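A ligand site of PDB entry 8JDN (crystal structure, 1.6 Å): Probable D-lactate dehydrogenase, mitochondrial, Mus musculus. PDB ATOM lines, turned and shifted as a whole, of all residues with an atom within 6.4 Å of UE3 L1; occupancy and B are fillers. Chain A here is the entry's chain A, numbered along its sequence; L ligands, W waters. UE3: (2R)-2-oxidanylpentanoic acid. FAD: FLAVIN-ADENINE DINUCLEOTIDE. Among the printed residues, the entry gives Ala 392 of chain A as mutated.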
ATOM      1  N   VAL A  88      -3.270  20.875  -1.650  1.00  0.00           N
ATOM      2  CA  VAL A  88      -2.147  21.785  -1.432  1.00  0.00           C
ATOM      3  C   VAL A  88      -0.870  21.322  -2.122  1.00  0.00           C
ATOM      4  O   VAL A  88       0.220  21.797  -1.781  1.00  0.00           O
ATOM      5  CB  VAL A  88      -1.901  22.004   0.078  1.00  0.00           C
ATOM      6  CG1 VAL A  88      -3.083  22.717   0.705  1.00  0.00           C
ATOM      7  CG2 VAL A  88      -1.662  20.689   0.772  1.00  0.00           C
ATOM      8  N   PRO A 145     -10.250  16.814   7.571  1.00  0.00           N
ATOM      9  CA  PRO A 145      -9.415  17.914   7.069  1.00  0.00           C
ATOM     10  C   PRO A 145     -10.069  19.248   7.366  1.00  0.00           C
ATOM     11  O   PRO A 145     -11.291  19.368   7.462  1.00  0.00           O
ATOM     12  CB  PRO A 145      -9.342  17.672   5.554  1.00  0.00           C
ATOM     13  CG  PRO A 145      -9.853  16.310   5.350  1.00  0.00           C
ATOM     14  CD  PRO A 145     -10.746  15.958   6.478  1.00  0.00           C
ATOM     15  N   GLY A 146      -9.232  20.282   7.520  1.00  0.00           N
ATOM     16  CA  GLY A 146      -9.748  21.580   7.897  1.00  0.00           C
ATOM     17  C   GLY A 146     -10.655  22.207   6.856  1.00  0.00           C
ATOM     18  O   GLY A 146     -11.557  22.984   7.198  1.00  0.00           O
ATOM     19  N   THR A 162      -7.741  15.742  12.299  1.00  0.00           N
ATOM     20  CA  THR A 162      -7.465  15.730  13.739  1.00  0.00           C
ATOM     21  C   THR A 162      -8.006  14.473  14.419  1.00  0.00           C
ATOM     22  O   THR A 162      -7.433  14.024  15.415  1.00  0.00           O
ATOM     23  CB  THR A 162      -8.035  16.977  14.435  1.00  0.00           C
ATOM     24  OG1 THR A 162      -9.463  16.884  14.502  1.00  0.00           O
ATOM     25  CG2 THR A 162      -7.657  18.235  13.695  1.00  0.00           C
ATOM     26  N   GLU A 264      -3.476  17.859  18.959  1.00  0.00           N
ATOM     27  CA  GLU A 264      -2.997  18.759  17.926  1.00  0.00           C
ATOM     28  C   GLU A 264      -1.992  19.728  18.500  1.00  0.00           C
ATOM     29  O   GLU A 264      -2.217  20.298  19.579  1.00  0.00           O
ATOM     30  CB  GLU A 264      -4.151  19.523  17.316  1.00  0.00           C
ATOM     31  CG  GLU A 264      -5.084  18.639  16.485  1.00  0.00           C
ATOM     32  CD  GLU A 264      -4.419  18.135  15.224  1.00  0.00           C
ATOM     33  OE1 GLU A 264      -4.542  16.921  14.914  1.00  0.00           O
ATOM     34  OE2 GLU A 264      -3.766  18.943  14.544  1.00  0.00           O
ATOM     35  N   ARG A 334      -8.672  25.716  14.820  1.00  0.00           N
ATOM     36  CA  ARG A 334      -7.652  24.778  14.381  1.00  0.00           C
ATOM     37  C   ARG A 334      -7.825  24.442  12.902  1.00  0.00           C
ATOM     38  O   ARG A 334      -6.857  24.447  12.138  1.00  0.00           O
ATOM     39  CB  ARG A 334      -7.718  23.508  15.239  1.00  0.00           C
ATOM     40  CG  ARG A 334      -6.976  22.304  14.662  1.00  0.00           C
ATOM     41  CD  ARG A 334      -5.480  22.574  14.567  1.00  0.00           C
ATOM     42  NE  ARG A 334      -4.795  21.469  13.904  1.00  0.00           N
ATOM     43  CZ  ARG A 334      -4.556  21.421  12.589  1.00  0.00           C
ATOM     44  NH1 ARG A 334      -4.925  22.429  11.809  1.00  0.00           N
ATOM     45  NH2 ARG A 334      -3.941  20.365  12.066  1.00  0.00           N
ATOM     46  N   HIS A 335      -9.060  24.139  12.489  1.00  0.00           N
ATOM     47  CA  HIS A 335      -9.308  23.787  11.096  1.00  0.00           C
ATOM     48  C   HIS A 335      -8.929  24.925  10.153  1.00  0.00           C
ATOM     49  O   HIS A 335      -8.600  24.674   8.992  1.00  0.00           O
ATOM     50  CB  HIS A 335     -10.776  23.415  10.920  1.00  0.00           C
ATOM     51  CG  HIS A 335     -11.104  22.040  11.408  1.00  0.00           C
ATOM     52  ND1 HIS A 335     -12.358  21.706  11.894  1.00  0.00           N
ATOM     53  CD2 HIS A 335     -10.362  20.914  11.485  1.00  0.00           C
ATOM     54  CE1 HIS A 335     -12.368  20.429  12.231  1.00  0.00           C
ATOM     55  NE2 HIS A 335     -11.166  19.920  11.990  1.00  0.00           N
ATOM     56  N   ASN A 336      -8.984  26.165  10.626  1.00  0.00           N
ATOM     57  CA  ASN A 336      -8.630  27.308   9.791  1.00  0.00           C
ATOM     58  C   ASN A 336      -7.187  27.768   9.967  1.00  0.00           C
ATOM     59  O   ASN A 336      -6.830  28.836   9.462  1.00  0.00           O
ATOM     60  CB  ASN A 336      -9.590  28.474  10.065  1.00  0.00           C
ATOM     61  CG  ASN A 336     -10.925  28.284   9.382  1.00  0.00           C
ATOM     62  OD1 ASN A 336     -11.052  28.529   8.184  1.00  0.00           O
ATOM     63  ND2 ASN A 336     -11.919  27.810  10.128  1.00  0.00           N
ATOM     64  N   ALA A 337      -6.334  26.965  10.618  1.00  0.00           N
ATOM     65  CA  ALA A 337      -4.929  27.344  10.827  1.00  0.00           C
ATOM     66  C   ALA A 337      -4.237  27.759   9.533  1.00  0.00           C
ATOM     67  O   ALA A 337      -3.446  28.706   9.518  1.00  0.00           O
ATOM     68  CB  ALA A 337      -4.171  26.182  11.474  1.00  0.00           C
ATOM     69  N   TRP A 338      -4.505  27.056   8.432  1.00  0.00           N
ATOM     70  CA  TRP A 338      -3.886  27.408   7.159  1.00  0.00           C
ATOM     71  C   TRP A 338      -4.204  28.851   6.780  1.00  0.00           C
ATOM     72  O   TRP A 338      -3.307  29.604   6.362  1.00  0.00           O
ATOM     73  CB  TRP A 338      -4.359  26.425   6.082  1.00  0.00           C
ATOM     74  CG  TRP A 338      -4.065  26.789   4.665  1.00  0.00           C
ATOM     75  CD1 TRP A 338      -4.923  27.364   3.763  1.00  0.00           C
ATOM     76  CD2 TRP A 338      -2.831  26.572   3.965  1.00  0.00           C
ATOM     77  NE1 TRP A 338      -4.289  27.512   2.547  1.00  0.00           N
ATOM     78  CE2 TRP A 338      -3.013  27.025   2.643  1.00  0.00           C
ATOM     79  CE3 TRP A 338      -1.592  26.024   4.323  1.00  0.00           C
ATOM     80  CZ2 TRP A 338      -2.002  26.982   1.689  1.00  0.00           C
ATOM     81  CZ3 TRP A 338      -0.583  25.972   3.370  1.00  0.00           C
ATOM     82  CH2 TRP A 338      -0.801  26.435   2.067  1.00  0.00           C
ATOM     83  N   SER A 352       3.200  24.077   2.220  1.00  0.00           N
ATOM     84  CA  SER A 352       3.155  23.308   3.449  1.00  0.00           C
ATOM     85  C   SER A 352       3.992  22.047   3.291  1.00  0.00           C
ATOM     86  O   SER A 352       3.863  21.339   2.285  1.00  0.00           O
ATOM     87  CB  SER A 352       1.730  22.924   3.838  1.00  0.00           C
ATOM     88  OG  SER A 352       1.726  22.176   5.055  1.00  0.00           O
ATOM     89  N   THR A 353       4.824  21.763   4.286  1.00  0.00           N
ATOM     90  CA  THR A 353       5.407  20.443   4.430  1.00  0.00           C
ATOM     91  C   THR A 353       4.424  19.554   5.182  1.00  0.00           C
ATOM     92  O   THR A 353       3.393  20.015   5.683  1.00  0.00           O
ATOM     93  CB  THR A 353       6.746  20.534   5.172  1.00  0.00           C
ATOM     94  OG1 THR A 353       6.531  20.990   6.504  1.00  0.00           O
ATOM     95  CG2 THR A 353       7.675  21.469   4.450  1.00  0.00           C
ATOM     96  N   ASP A 354       4.729  18.253   5.270  1.00  0.00           N
ATOM     97  CA  ASP A 354       3.759  17.299   5.781  1.00  0.00           C
ATOM     98  C   ASP A 354       4.425  16.007   6.242  1.00  0.00           C
ATOM     99  O   ASP A 354       3.860  14.930   6.082  1.00  0.00           O
ATOM    100  CB  ASP A 354       2.736  16.988   4.674  1.00  0.00           C
ATOM    101  CG  ASP A 354       1.577  16.117   5.157  1.00  0.00           C
ATOM    102  OD1 ASP A 354       1.135  16.229   6.316  1.00  0.00           O
ATOM    103  OD2 ASP A 354       1.072  15.357   4.310  1.00  0.00           O
ATOM    104  N   VAL A 383       1.940  23.508  12.732  1.00  0.00           N
ATOM    105  CA  VAL A 383       0.718  22.934  13.266  1.00  0.00           C
ATOM    106  C   VAL A 383       0.736  21.464  12.891  1.00  0.00           C
ATOM    107  O   VAL A 383       1.294  21.078  11.864  1.00  0.00           O
ATOM    108  CB  VAL A 383      -0.540  23.666  12.724  1.00  0.00           C
ATOM    109  CG1 VAL A 383      -0.691  23.424  11.205  1.00  0.00           C
ATOM    110  CG2 VAL A 383      -1.785  23.252  13.490  1.00  0.00           C
ATOM    111  N   GLY A 384       0.186  20.606  13.748  1.00  0.00           N
ATOM    112  CA  GLY A 384       0.325  19.211  13.378  1.00  0.00           C
ATOM    113  C   GLY A 384      -0.503  18.168  14.084  1.00  0.00           C
ATOM    114  O   GLY A 384      -0.777  18.264  15.275  1.00  0.00           O
ATOM    115  N   HIS A 385      -0.882  17.138  13.308  1.00  0.00           N
ATOM    116  CA  HIS A 385      -1.466  15.907  13.812  1.00  0.00           C
ATOM    117  C   HIS A 385      -0.390  15.074  14.483  1.00  0.00           C
ATOM    118  O   HIS A 385      -0.034  13.979  14.004  1.00  0.00           O
ATOM    119  CB  HIS A 385      -2.110  15.111  12.653  1.00  0.00           C
ATOM    120  CG  HIS A 385      -3.026  15.920  11.781  1.00  0.00           C
ATOM    121  ND1 HIS A 385      -4.084  16.654  12.273  1.00  0.00           N
ATOM    122  CD2 HIS A 385      -3.043  16.095  10.437  1.00  0.00           C
ATOM    123  CE1 HIS A 385      -4.723  17.232  11.268  1.00  0.00           C
ATOM    124  NE2 HIS A 385      -4.108  16.917  10.142  1.00  0.00           N
ATOM    125  N   ALA A 392       2.849  19.847   9.974  1.00  0.00           N
ATOM    126  CA  ALA A 392       2.966  20.730   8.823  1.00  0.00           C
ATOM    127  C   ALA A 392       3.755  21.970   9.215  1.00  0.00           C
ATOM    128  O   ALA A 392       3.498  22.556  10.270  1.00  0.00           O
ATOM    129  CB  ALA A 392       1.591  21.130   8.299  1.00  0.00           C
ATOM    130  N   ILE A 394       4.053  25.549   7.669  1.00  0.00           N
ATOM    131  CA  ILE A 394       3.395  26.423   6.707  1.00  0.00           C
ATOM    132  C   ILE A 394       4.304  27.610   6.456  1.00  0.00           C
ATOM    133  O   ILE A 394       4.585  28.398   7.379  1.00  0.00           O
ATOM    134  CB  ILE A 394       2.020  26.882   7.209  1.00  0.00           C
ATOM    135  CG1 ILE A 394       1.100  25.676   7.449  1.00  0.00           C
ATOM    136  CG2 ILE A 394       1.396  27.859   6.209  1.00  0.00           C
ATOM    137  CD1 ILE A 394      -0.165  26.020   8.225  1.00  0.00           C
ATOM    138  N   GLU A 429      -0.290  12.928   4.705  1.00  0.00           N
ATOM    139  CA  GLU A 429      -1.686  13.003   4.300  1.00  0.00           C
ATOM    140  C   GLU A 429      -1.960  13.855   3.045  1.00  0.00           C
ATOM    141  O   GLU A 429      -2.926  13.576   2.330  1.00  0.00           O
ATOM    142  CB  GLU A 429      -2.515  13.529   5.487  1.00  0.00           C
ATOM    143  CG  GLU A 429      -2.067  14.910   5.985  1.00  0.00           C
ATOM    144  CD  GLU A 429      -2.966  15.524   7.052  1.00  0.00           C
ATOM    145  OE1 GLU A 429      -3.926  14.862   7.520  1.00  0.00           O
ATOM    146  OE2 GLU A 429      -2.739  16.697   7.411  1.00  0.00           O
ATOM    147  N   HIS A 430      -1.142  14.876   2.772  1.00  0.00           N
ATOM    148  CA  HIS A 430      -1.477  15.797   1.678  1.00  0.00           C
ATOM    149  C   HIS A 430      -1.274  15.166   0.307  1.00  0.00           C
ATOM    150  O   HIS A 430      -1.961  15.542  -0.648  1.00  0.00           O
ATOM    151  CB  HIS A 430      -0.629  17.058   1.747  1.00  0.00           C
ATOM    152  CG  HIS A 430      -0.918  17.891   2.954  1.00  0.00           C
ATOM    153  ND1 HIS A 430       0.013  18.769   3.468  1.00  0.00           N
ATOM    154  CD2 HIS A 430      -2.011  17.989   3.737  1.00  0.00           C
ATOM    155  CE1 HIS A 430      -0.499  19.373   4.527  1.00  0.00           C
ATOM    156  NE2 HIS A 430      -1.730  18.915   4.712  1.00  0.00           N
HETATM  157  CAA UE3 L   1      -3.936  21.149   8.666  1.00  0.00           C
HETATM  158  CAB UE3 L   1      -3.378  21.309   7.266  1.00  0.00           C
HETATM  159  CAC UE3 L   1      -2.386  22.464   7.226  1.00  0.00           C
HETATM  160  CAD UE3 L   1      -1.764  22.578   5.833  1.00  0.00           C
HETATM  161  CAE UE3 L   1      -2.848  22.718   4.762  1.00  0.00           C
HETATM  162  OAF UE3 L   1      -3.522  20.219   9.394  1.00  0.00           O
HETATM  163  OAG UE3 L   1      -4.828  21.953   9.091  1.00  0.00           O
HETATM  164  OAH UE3 L   1      -2.713  20.105   6.952  1.00  0.00           O
HETATM  165  PA  FAD L   2      -8.717  18.681  -5.168  1.00  0.00           P
HETATM  166  O1A FAD L   2      -7.730  19.768  -4.945  1.00  0.00           O
HETATM  167  O2A FAD L   2      -9.946  18.960  -5.977  1.00  0.00           O
HETATM  168  O5B FAD L   2      -7.940  17.484  -5.809  1.00  0.00           O
HETATM  169  C5B FAD L   2      -6.807  16.896  -5.128  1.00  0.00           C
HETATM  170  C4B FAD L   2      -6.208  15.787  -5.954  1.00  0.00           C
HETATM  171  O4B FAD L   2      -7.110  14.656  -5.975  1.00  0.00           O
HETATM  172  C3B FAD L   2      -5.935  16.131  -7.416  1.00  0.00           C
HETATM  173  O3B FAD L   2      -4.789  15.428  -7.897  1.00  0.00           O
HETATM  174  C2B FAD L   2      -7.224  15.682  -8.107  1.00  0.00           C
HETATM  175  O2B FAD L   2      -7.049  15.336  -9.479  1.00  0.00           O
HETATM  176  C1B FAD L   2      -7.591  14.448  -7.293  1.00  0.00           C
HETATM  177  N9A FAD L   2      -9.023  14.184  -7.190  1.00  0.00           N
HETATM  178  C8A FAD L   2      -9.995  14.977  -6.629  1.00  0.00           C
HETATM  179  N7A FAD L   2     -11.191  14.451  -6.655  1.00  0.00           N
HETATM  180  C5A FAD L   2     -11.001  13.219  -7.268  1.00  0.00           C
HETATM  181  C6A FAD L   2     -11.881  12.170  -7.592  1.00  0.00           C
HETATM  182  N6A FAD L   2     -13.184  12.180  -7.323  1.00  0.00           N
HETATM  183  N1A FAD L   2     -11.350  11.075  -8.208  1.00  0.00           N
HETATM  184  C2A FAD L   2     -10.043  11.055  -8.462  1.00  0.00           C
HETATM  185  N3A FAD L   2      -9.122  11.985  -8.203  1.00  0.00           N
HETATM  186  C4A FAD L   2      -9.669  13.043  -7.596  1.00  0.00           C
HETATM  187  N1  FAD L   2      -5.630  17.457   3.979  1.00  0.00           N
HETATM  188  C2  FAD L   2      -5.467  16.458   4.896  1.00  0.00           C
HETATM  189  O2  FAD L   2      -5.181  15.299   4.553  1.00  0.00           O
HETATM  190  N3  FAD L   2      -5.593  16.739   6.240  1.00  0.00           N
HETATM  191  C4  FAD L   2      -5.929  17.959   6.800  1.00  0.00           C
HETATM  192  O4  FAD L   2      -6.005  18.084   8.026  1.00  0.00           O
HETATM  193  C4X FAD L   2      -6.116  19.011   5.826  1.00  0.00           C
HETATM  194  N5  FAD L   2      -6.440  20.227   6.253  1.00  0.00           N
HETATM  195  C5X FAD L   2      -6.620  21.229   5.321  1.00  0.00           C
HETATM  196  C6  FAD L   2      -6.966  22.503   5.753  1.00  0.00           C
HETATM  197  C7  FAD L   2      -7.147  23.538   4.846  1.00  0.00           C
HETATM  198  C7M FAD L   2      -7.523  24.908   5.360  1.00  0.00           C
HETATM  199  C8  FAD L   2      -6.992  23.299   3.473  1.00  0.00           C
HETATM  200  C8M FAD L   2      -7.190  24.402   2.466  1.00  0.00           C
HETATM  201  C9  FAD L   2      -6.664  22.029   3.034  1.00  0.00           C
HETATM  202  C9A FAD L   2      -6.461  20.989   3.937  1.00  0.00           C
HETATM  203  N10 FAD L   2      -6.145  19.681   3.511  1.00  0.00           N
HETATM  204  C10 FAD L   2      -5.951  18.675   4.428  1.00  0.00           C
HETATM  205  C1' FAD L   2      -5.888  19.394   2.092  1.00  0.00           C
HETATM  206  C2' FAD L   2      -7.124  19.045   1.274  1.00  0.00           C
HETATM  207  O2' FAD L   2      -8.291  19.589   1.880  1.00  0.00           O
HETATM  208  C3' FAD L   2      -7.239  17.535   1.141  1.00  0.00           C
HETATM  209  O3' FAD L   2      -6.082  17.070   0.456  1.00  0.00           O
HETATM  210  C4' FAD L   2      -8.505  17.088   0.415  1.00  0.00           C
HETATM  211  O4' FAD L   2      -8.563  15.662   0.454  1.00  0.00           O
HETATM  212  C5' FAD L   2      -8.542  17.579  -1.028  1.00  0.00           C
HETATM  213  O5' FAD L   2      -9.838  17.308  -1.590  1.00  0.00           O
HETATM  214  P   FAD L   2     -10.372  18.141  -2.816  1.00  0.00           P
HETATM  215  O1P FAD L   2     -11.600  17.497  -3.457  1.00  0.00           O
HETATM  216  O2P FAD L   2     -10.544  19.579  -2.388  1.00  0.00           O
HETATM  217  O3P FAD L   2      -9.116  18.009  -3.787  1.00  0.00           O
HETATM  218  O   HOH W   1      -7.402  21.053   9.931  1.00  0.00           O
HETATM  219  O   HOH W   2      -0.395  17.836   7.625  1.00  0.00           O
HETATM  220  O   HOH W   3      -5.766  24.507   8.549  1.00  0.00           O
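Trp 338 touches UE3 L1. Ser 352 touches UE3 L1 (OG to CAD, 3.6 Å). Hydrophobic or aromatic side chains that line UE3 L1: Trp 338, His 385 and His 430. Within 4 Å of UE3 L1: Arg 334, Trp 338, Ser 352, His 385, Glu 429 and His 430. The nearest printed residue that does not touch UE3 L1 is Val 88 (4.1 Å).
N of Gly 146 lies within hydrogen-bond range of N5 of FAD L2, 3.1 Å away. OAH of UE3 L1 sits at hydrogen-bond distance from OE2 of Glu 429 (3.4 Å). A ring nitrogen (NE2) of His 385 is in hydrogen-bond range of an oxygen (O4) of FAD L2 (3.1 Å). A nitrogen (N3) of FAD L2 lies within hydrogen-bond range of the side-chain carboxylate (OE1) of Glu 429. A ring nitrogen (NE2) of His 385 lies within hydrogen-bond range of an oxygen (OAF) of UE3 L1. OAF of UE3 L1 lies within salt-bridge range of NH2 of Arg 334 (2.7 Å). A ring nitrogen (NE2) of His 430 is in hydrogen-bond range of an oxygen (OAH) of UE3 L1 (2.7 Å).
Water W3 lies within hydrogen-bond range of an oxygen (OAG) of UE3 L1 (2.8 Å), the backbone NH (N) of Trp 338 (2.8 Å), the backbone carbonyl oxygen (O) of His 335 (2.9 Å) and the backbone NH (N) of Ala 337 (3.3 Å). Water W1 lies within hydrogen-bond range of OAG of UE3 L1 (2.9 Å), N of Gly 146 (3.1 Å) and NH1 of Arg 334 (3.4 Å). Water W2 lies within hydrogen-bond range of OD1 of Asp 354 (2.6 Å), OE2 of Glu 429 (2.6 Å), OAH of UE3 L1 (3.3 Å) and NE2 of His 430 (3.4 Å).
OE2 of Glu 264 is in salt-bridge range of NE of Arg 334 (2.8 Å). The side-chain carboxylate (OE2) of Glu 429 sits at hydrogen-bond distance from a ring nitrogen (NE2) of His 385 (3.1 Å). The backbone NH (N) of Glu 429 sits at hydrogen-bond distance from the side-chain carboxylate (OD2) of Asp 354 (2.8 Å). A ring nitrogen (ND1) of His 385 is in hydrogen-bond range of the side-chain carboxylate (OE1) of Glu 264 (2.7 Å). The side-chain carboxylate (OD2) of Asp 354 is in hydrogen-bond range of the backbone NH (N) of His 430 (2.7 Å).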
